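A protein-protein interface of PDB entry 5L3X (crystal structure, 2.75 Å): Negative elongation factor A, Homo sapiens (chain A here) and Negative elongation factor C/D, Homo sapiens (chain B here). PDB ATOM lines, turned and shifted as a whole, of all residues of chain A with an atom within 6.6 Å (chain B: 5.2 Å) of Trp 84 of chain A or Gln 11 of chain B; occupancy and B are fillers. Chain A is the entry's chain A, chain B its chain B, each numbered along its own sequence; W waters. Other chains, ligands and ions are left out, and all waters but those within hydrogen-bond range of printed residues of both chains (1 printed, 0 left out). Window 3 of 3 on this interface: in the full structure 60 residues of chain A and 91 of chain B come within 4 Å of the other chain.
The backbone NH (N) of Phe 16 of chain B lies close to the backbone carbonyl oxygen (O) of Ala 9 of chain B.
Printed residues of chain B that touch a printed residue of chain A: Cys 10, Gln 11, Gln 12, Leu 13, Phe 16, His 51, Thr 52 and Phe 55. Printed residues of chain A that touch a printed residue of chain B: Leu 49, Pro 83, Trp 84 and Met 87. Hydrophobic or aromatic side chains of chain A within 4 Å of the printed part of chain B: Leu 49, Pro 83, Trp 84 and Met 87. Among the printed residues, 12 pairs touch across the chains.
Water W1 bridges the side-chain carboxylate (OD1) of Asp 82 of chain A (2.4 Å) and the backbone carbonyl oxygen (O) of Gln 11 of chain B (3.1 Å).
His 51 of chain B touches Leu 49 of chain A. Leu 13 of chain B touches Pro 83 of chain A. NE1 of Trp 84 of chain A touches C of Gln 12 of chain B, 3.9 Å away. Leu 13 of chain B touches Trp 84 of chain A (N to NE1, 3.6 Å). Trp 84 of chain A touches Phe 16 of chain B (CH2 to CD1, 3.7 Å). CE3 of Trp 84 of chain A touches ND1 of His 51 of chain B (3.7 Å). CH2 of Trp 84 of chain A touches CG2 of Thr 52 of chain B, at 3.9 Å. Phe 55 of chain B touches Trp 84 of chain A. Met 87 of chain A touches Leu 13 of chain B. Phe 55 of chain B touches Met 87 of chain A.
O of Cys 10 of chain B is in hydrogen-bond range of NE1 of Trp 84 of chain A (2.7 Å). NE1 of Trp 84 of chain A sits at hydrogen-bond distance from O of Gln 11 of chain B, 3.4 Å away.
Of chain B, only Cys 10 (2.7 Å), Gln 11 (3.4 Å), Gln 12 (3.9 Å), Leu 13 (3.6 Å), Phe 16 (3.7 Å), His 51 (3.7 Å), Thr 52 (3.9 Å) and Phe 55 (3.9 Å) come within 4 Å of Trp 84 of chain A. Of chain A, only Trp 84 (3.4 Å) comes within 4 Å of Gln 11 of chain B. Of the printed residues of chain A, Phe 16 of chain B touches Trp 84. Of the printed residues of chain A, Phe 55 of chain B touches Trp 84 (3.9 Å) and Met 87 (3.4 Å). Thr 8 of chain B touches none of the printed residues of chain A. The nearest printed residue of chain B that does not touch Trp 84 of chain A is Ala 9 of chain B (5.6 Å).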
ATOM      1  N   SER A  45     -26.364  25.043  -0.642  1.00  0.00           N
ATOM      2  CA  SER A  45     -26.184  25.124   0.798  1.00  0.00           C
ATOM      3  C   SER A  45     -25.110  24.157   1.265  1.00  0.00           C
ATOM      4  O   SER A  45     -24.271  24.508   2.099  1.00  0.00           O
ATOM      5  CB  SER A  45     -27.503  24.847   1.527  1.00  0.00           C
ATOM      6  OG  SER A  45     -28.473  25.831   1.200  1.00  0.00           O
ATOM      7  N   LEU A  49     -21.875  25.161   3.416  1.00  0.00           N
ATOM      8  CA  LEU A  49     -21.677  24.599   4.744  1.00  0.00           C
ATOM      9  C   LEU A  49     -20.315  23.925   4.865  1.00  0.00           C
ATOM     10  O   LEU A  49     -19.748  23.841   5.954  1.00  0.00           O
ATOM     11  CB  LEU A  49     -22.790  23.602   5.072  1.00  0.00           C
ATOM     12  CG  LEU A  49     -24.177  24.218   5.240  1.00  0.00           C
ATOM     13  CD1 LEU A  49     -25.221  23.141   5.523  1.00  0.00           C
ATOM     14  CD2 LEU A  49     -24.151  25.269   6.341  1.00  0.00           C
ATOM     15  N   LEU A  52     -17.871  27.244   4.849  1.00  0.00           N
ATOM     16  CA  LEU A  52     -17.838  27.977   6.112  1.00  0.00           C
ATOM     17  C   LEU A  52     -17.150  27.188   7.221  1.00  0.00           C
ATOM     18  O   LEU A  52     -16.352  27.739   7.983  1.00  0.00           O
ATOM     19  CB  LEU A  52     -19.257  28.355   6.548  1.00  0.00           C
ATOM     20  CG  LEU A  52     -20.004  29.375   5.686  1.00  0.00           C
ATOM     21  CD1 LEU A  52     -21.489  29.327   5.992  1.00  0.00           C
ATOM     22  CD2 LEU A  52     -19.456  30.776   5.902  1.00  0.00           C
ATOM     23  N   SER A  81     -30.514  32.354   2.406  1.00  0.00           N
ATOM     24  CA  SER A  81     -31.903  31.923   2.533  1.00  0.00           C
ATOM     25  C   SER A  81     -32.028  30.643   3.355  1.00  0.00           C
ATOM     26  O   SER A  81     -33.060  30.387   3.977  1.00  0.00           O
ATOM     27  CB  SER A  81     -32.526  31.713   1.151  1.00  0.00           C
ATOM     28  OG  SER A  81     -31.874  30.664   0.457  1.00  0.00           O
ATOM     29  N   ASP A  82     -30.973  29.838   3.358  1.00  0.00           N
ATOM     30  CA  ASP A  82     -30.989  28.590   4.107  1.00  0.00           C
ATOM     31  C   ASP A  82     -30.806  28.868   5.600  1.00  0.00           C
ATOM     32  O   ASP A  82     -29.870  29.555   6.000  1.00  0.00           O
ATOM     33  CB  ASP A  82     -29.905  27.638   3.597  1.00  0.00           C
ATOM     34  CG  ASP A  82     -30.063  26.234   4.144  1.00  0.00           C
ATOM     35  OD1 ASP A  82     -31.218  25.784   4.285  1.00  0.00           O
ATOM     36  OD2 ASP A  82     -29.041  25.583   4.442  1.00  0.00           O
ATOM     37  N   PRO A  83     -31.733  28.366   6.429  1.00  0.00           N
ATOM     38  CA  PRO A  83     -31.593  28.512   7.882  1.00  0.00           C
ATOM     39  C   PRO A  83     -30.311  27.890   8.449  1.00  0.00           C
ATOM     40  O   PRO A  83     -29.793  28.397   9.450  1.00  0.00           O
ATOM     41  CB  PRO A  83     -32.839  27.802   8.435  1.00  0.00           C
ATOM     42  CG  PRO A  83     -33.581  27.248   7.245  1.00  0.00           C
ATOM     43  CD  PRO A  83     -33.096  27.965   6.042  1.00  0.00           C
ATOM     44  N   TRP A  84     -29.802  26.827   7.830  1.00  0.00           N
ATOM     45  CA  TRP A  84     -28.553  26.217   8.292  1.00  0.00           C
ATOM     46  C   TRP A  84     -27.358  27.129   8.031  1.00  0.00           C
ATOM     47  O   TRP A  84     -26.469  27.258   8.873  1.00  0.00           O
ATOM     48  CB  TRP A  84     -28.319  24.861   7.624  1.00  0.00           C
ATOM     49  CG  TRP A  84     -29.003  23.709   8.300  1.00  0.00           C
ATOM     50  CD1 TRP A  84     -30.047  22.978   7.817  1.00  0.00           C
ATOM     51  CD2 TRP A  84     -28.678  23.147   9.579  1.00  0.00           C
ATOM     52  NE1 TRP A  84     -30.397  21.998   8.712  1.00  0.00           N
ATOM     53  CE2 TRP A  84     -29.572  22.079   9.801  1.00  0.00           C
ATOM     54  CE3 TRP A  84     -27.721  23.442  10.556  1.00  0.00           C
ATOM     55  CZ2 TRP A  84     -29.537  21.306  10.961  1.00  0.00           C
ATOM     56  CZ3 TRP A  84     -27.691  22.674  11.708  1.00  0.00           C
ATOM     57  CH2 TRP A  84     -28.593  21.618  11.899  1.00  0.00           C
ATOM     58  N   VAL A  85     -27.333  27.753   6.858  1.00  0.00           N
ATOM     59  CA  VAL A  85     -26.262  28.679   6.519  1.00  0.00           C
ATOM     60  C   VAL A  85     -26.288  29.883   7.459  1.00  0.00           C
ATOM     61  O   VAL A  85     -25.239  30.348   7.904  1.00  0.00           O
ATOM     62  CB  VAL A  85     -26.363  29.152   5.050  1.00  0.00           C
ATOM     63  CG1 VAL A  85     -25.245  30.132   4.726  1.00  0.00           C
ATOM     64  CG2 VAL A  85     -26.315  27.961   4.102  1.00  0.00           C
ATOM     65  N   LEU A  86     -27.490  30.362   7.780  1.00  0.00           N
ATOM     66  CA  LEU A  86     -27.653  31.509   8.677  1.00  0.00           C
ATOM     67  C   LEU A  86     -27.141  31.211  10.087  1.00  0.00           C
ATOM     68  O   LEU A  86     -26.465  32.037  10.701  1.00  0.00           O
ATOM     69  CB  LEU A  86     -29.113  31.936   8.743  1.00  0.00           C
ATOM     70  CG  LEU A  86     -29.759  32.496   7.471  1.00  0.00           C
ATOM     71  CD1 LEU A  86     -31.256  32.650   7.661  1.00  0.00           C
ATOM     72  CD2 LEU A  86     -29.127  33.825   7.088  1.00  0.00           C
ATOM     73  N   MET A  87     -27.466  30.025  10.590  1.00  0.00           N
ATOM     74  CA  MET A  87     -27.057  29.614  11.925  1.00  0.00           C
ATOM     75  C   MET A  87     -25.542  29.491  12.036  1.00  0.00           C
ATOM     76  O   MET A  87     -24.952  29.883  13.039  1.00  0.00           O
ATOM     77  CB  MET A  87     -27.713  28.284  12.299  1.00  0.00           C
ATOM     78  CG  MET A  87     -27.566  27.914  13.762  1.00  0.00           C
ATOM     79  SD  MET A  87     -28.307  29.129  14.873  1.00  0.00           S
ATOM     80  CE  MET A  87     -30.044  28.876  14.539  1.00  0.00           C
ATOM     81  N   VAL A  88     -24.917  28.944  11.000  1.00  0.00           N
ATOM     82  CA  VAL A  88     -23.471  28.750  10.994  1.00  0.00           C
ATOM     83  C   VAL A  88     -22.749  30.094  10.887  1.00  0.00           C
ATOM     84  O   VAL A  88     -21.725  30.315  11.537  1.00  0.00           O
ATOM     85  CB  VAL A  88     -23.041  27.807   9.843  1.00  0.00           C
ATOM     86  CG1 VAL A  88     -21.536  27.826   9.653  1.00  0.00           C
ATOM     87  CG2 VAL A  88     -23.529  26.390  10.113  1.00  0.00           C
ATOM     88  N   ALA A  89     -23.304  31.000  10.089  1.00  0.00           N
ATOM     89  CA  ALA A  89     -22.746  32.338   9.939  1.00  0.00           C
ATOM     90  C   ALA A  89     -22.774  33.127  11.246  1.00  0.00           C
ATOM     91  O   ALA A  89     -21.967  34.037  11.442  1.00  0.00           O
ATOM     92  CB  ALA A  89     -23.494  33.098   8.860  1.00  0.00           C
ATOM     93  N   SER B   7     -31.049  11.653   7.788  1.00  0.00           N
ATOM     94  CA  SER B   7     -31.106  12.653   6.721  1.00  0.00           C
ATOM     95  C   SER B   7     -32.289  13.613   6.870  1.00  0.00           C
ATOM     96  O   SER B   7     -32.119  14.834   6.819  1.00  0.00           O
ATOM     97  CB  SER B   7     -31.177  11.969   5.355  1.00  0.00           C
ATOM     98  OG  SER B   7     -30.028  11.177   5.113  1.00  0.00           O
ATOM     99  N   THR B   8     -33.482  13.054   7.054  1.00  0.00           N
ATOM    100  CA  THR B   8     -34.697  13.856   7.181  1.00  0.00           C
ATOM    101  C   THR B   8     -34.630  14.801   8.378  1.00  0.00           C
ATOM    102  O   THR B   8     -34.972  15.981   8.275  1.00  0.00           O
ATOM    103  CB  THR B   8     -35.951  12.965   7.317  1.00  0.00           C
ATOM    104  OG1 THR B   8     -36.090  12.141   6.150  1.00  0.00           O
ATOM    105  CG2 THR B   8     -37.199  13.819   7.493  1.00  0.00           C
ATOM    106  N   ALA B   9     -34.172  14.277   9.509  1.00  0.00           N
ATOM    107  CA  ALA B   9     -34.114  15.040  10.754  1.00  0.00           C
ATOM    108  C   ALA B   9     -33.119  16.205  10.708  1.00  0.00           C
ATOM    109  O   ALA B   9     -33.203  17.117  11.523  1.00  0.00           O
ATOM    110  CB  ALA B   9     -33.779  14.112  11.916  1.00  0.00           C
ATOM    111  N   CYS B  10     -32.190  16.174   9.754  1.00  0.00           N
ATOM    112  CA  CYS B  10     -31.133  17.182   9.682  1.00  0.00           C
ATOM    113  C   CYS B  10     -31.354  18.215   8.585  1.00  0.00           C
ATOM    114  O   CYS B  10     -30.730  19.276   8.594  1.00  0.00           O
ATOM    115  CB  CYS B  10     -29.770  16.517   9.466  1.00  0.00           C
ATOM    116  SG  CYS B  10     -29.161  15.573  10.873  1.00  0.00           S
ATOM    117  N   GLN B  11     -32.233  17.899   7.640  1.00  0.00           N
ATOM    118  CA  GLN B  11     -32.451  18.758   6.480  1.00  0.00           C
ATOM    119  C   GLN B  11     -33.072  20.097   6.875  1.00  0.00           C
ATOM    120  O   GLN B  11     -32.723  21.138   6.315  1.00  0.00           O
ATOM    121  CB  GLN B  11     -33.333  18.046   5.450  1.00  0.00           C
ATOM    122  CG  GLN B  11     -33.479  18.797   4.135  1.00  0.00           C
ATOM    123  CD  GLN B  11     -34.174  17.981   3.062  1.00  0.00           C
ATOM    124  OE1 GLN B  11     -34.761  16.934   3.339  1.00  0.00           O
ATOM    125  NE2 GLN B  11     -34.105  18.458   1.824  1.00  0.00           N
ATOM    126  N   GLN B  12     -33.990  20.062   7.838  1.00  0.00           N
ATOM    127  CA  GLN B  12     -34.645  21.276   8.318  1.00  0.00           C
ATOM    128  C   GLN B  12     -34.170  21.637   9.725  1.00  0.00           C
ATOM    129  O   GLN B  12     -34.276  20.833  10.650  1.00  0.00           O
ATOM    130  CB  GLN B  12     -36.169  21.107   8.309  1.00  0.00           C
ATOM    131  CG  GLN B  12     -36.747  20.583   6.995  1.00  0.00           C
ATOM    132  CD  GLN B  12     -36.691  21.603   5.870  1.00  0.00           C
ATOM    133  OE1 GLN B  12     -36.580  22.806   6.110  1.00  0.00           O
ATOM    134  NE2 GLN B  12     -36.767  21.123   4.632  1.00  0.00           N
ATOM    135  N   LEU B  13     -33.649  22.852   9.876  1.00  0.00           N
ATOM    136  CA  LEU B  13     -33.132  23.327  11.160  1.00  0.00           C
ATOM    137  C   LEU B  13     -34.203  23.304  12.245  1.00  0.00           C
ATOM    138  O   LEU B  13     -33.927  22.988  13.404  1.00  0.00           O
ATOM    139  CB  LEU B  13     -32.573  24.742  11.014  1.00  0.00           C
ATOM    140  CG  LEU B  13     -32.033  25.410  12.280  1.00  0.00           C
ATOM    141  CD1 LEU B  13     -30.893  24.600  12.882  1.00  0.00           C
ATOM    142  CD2 LEU B  13     -31.576  26.826  11.985  1.00  0.00           C
ATOM    143  N   PHE B  16     -34.657  19.640  13.294  1.00  0.00           N
ATOM    144  CA  PHE B  16     -33.474  19.214  14.028  1.00  0.00           C
ATOM    145  C   PHE B  16     -33.479  19.792  15.441  1.00  0.00           C
ATOM    146  O   PHE B  16     -33.111  19.114  16.394  1.00  0.00           O
ATOM    147  CB  PHE B  16     -32.209  19.636  13.282  1.00  0.00           C
ATOM    148  CG  PHE B  16     -30.931  19.291  14.000  1.00  0.00           C
ATOM    149  CD1 PHE B  16     -30.343  20.193  14.871  1.00  0.00           C
ATOM    150  CD2 PHE B  16     -30.315  18.069  13.795  1.00  0.00           C
ATOM    151  CE1 PHE B  16     -29.168  19.881  15.534  1.00  0.00           C
ATOM    152  CE2 PHE B  16     -29.137  17.753  14.454  1.00  0.00           C
ATOM    153  CZ  PHE B  16     -28.565  18.662  15.324  1.00  0.00           C
ATOM    154  N   HIS B  51     -21.635  20.718  10.117  1.00  0.00           N
ATOM    155  CA  HIS B  51     -22.472  21.868  10.448  1.00  0.00           C
ATOM    156  C   HIS B  51     -23.506  21.503  11.506  1.00  0.00           C
ATOM    157  O   HIS B  51     -23.823  22.314  12.373  1.00  0.00           O
ATOM    158  CB  HIS B  51     -23.162  22.429   9.200  1.00  0.00           C
ATOM    159  CG  HIS B  51     -23.990  21.428   8.459  1.00  0.00           C
ATOM    160  ND1 HIS B  51     -25.364  21.392   8.545  1.00  0.00           N
ATOM    161  CD2 HIS B  51     -23.640  20.435   7.608  1.00  0.00           C
ATOM    162  CE1 HIS B  51     -25.825  20.417   7.783  1.00  0.00           C
ATOM    163  NE2 HIS B  51     -24.799  19.819   7.206  1.00  0.00           N
ATOM    164  N   THR B  52     -24.024  20.279  11.445  1.00  0.00           N
ATOM    165  CA  THR B  52     -24.952  19.805  12.467  1.00  0.00           C
ATOM    166  C   THR B  52     -24.223  19.609  13.792  1.00  0.00           C
ATOM    167  O   THR B  52     -24.761  19.908  14.857  1.00  0.00           O
ATOM    168  CB  THR B  52     -25.635  18.486  12.057  1.00  0.00           C
ATOM    169  OG1 THR B  52     -24.650  17.451  11.931  1.00  0.00           O
ATOM    170  CG2 THR B  52     -26.382  18.656  10.732  1.00  0.00           C
ATOM    171  N   PHE B  55     -23.617  23.204  15.373  1.00  0.00           N
ATOM    172  CA  PHE B  55     -24.812  23.805  15.974  1.00  0.00           C
ATOM    173  C   PHE B  55     -25.161  23.180  17.321  1.00  0.00           C
ATOM    174  O   PHE B  55     -25.394  23.889  18.298  1.00  0.00           O
ATOM    175  CB  PHE B  55     -26.011  23.694  15.026  1.00  0.00           C
ATOM    176  CG  PHE B  55     -27.321  24.115  15.650  1.00  0.00           C
ATOM    177  CD1 PHE B  55     -27.504  25.411  16.110  1.00  0.00           C
ATOM    178  CD2 PHE B  55     -28.365  23.212  15.782  1.00  0.00           C
ATOM    179  CE1 PHE B  55     -28.698  25.799  16.689  1.00  0.00           C
ATOM    180  CE2 PHE B  55     -29.568  23.594  16.362  1.00  0.00           C
ATOM    181  CZ  PHE B  55     -29.732  24.889  16.815  1.00  0.00           C
HETATM  182  O   HOH W   1     -32.236  23.593   4.454  1.00  0.00           O
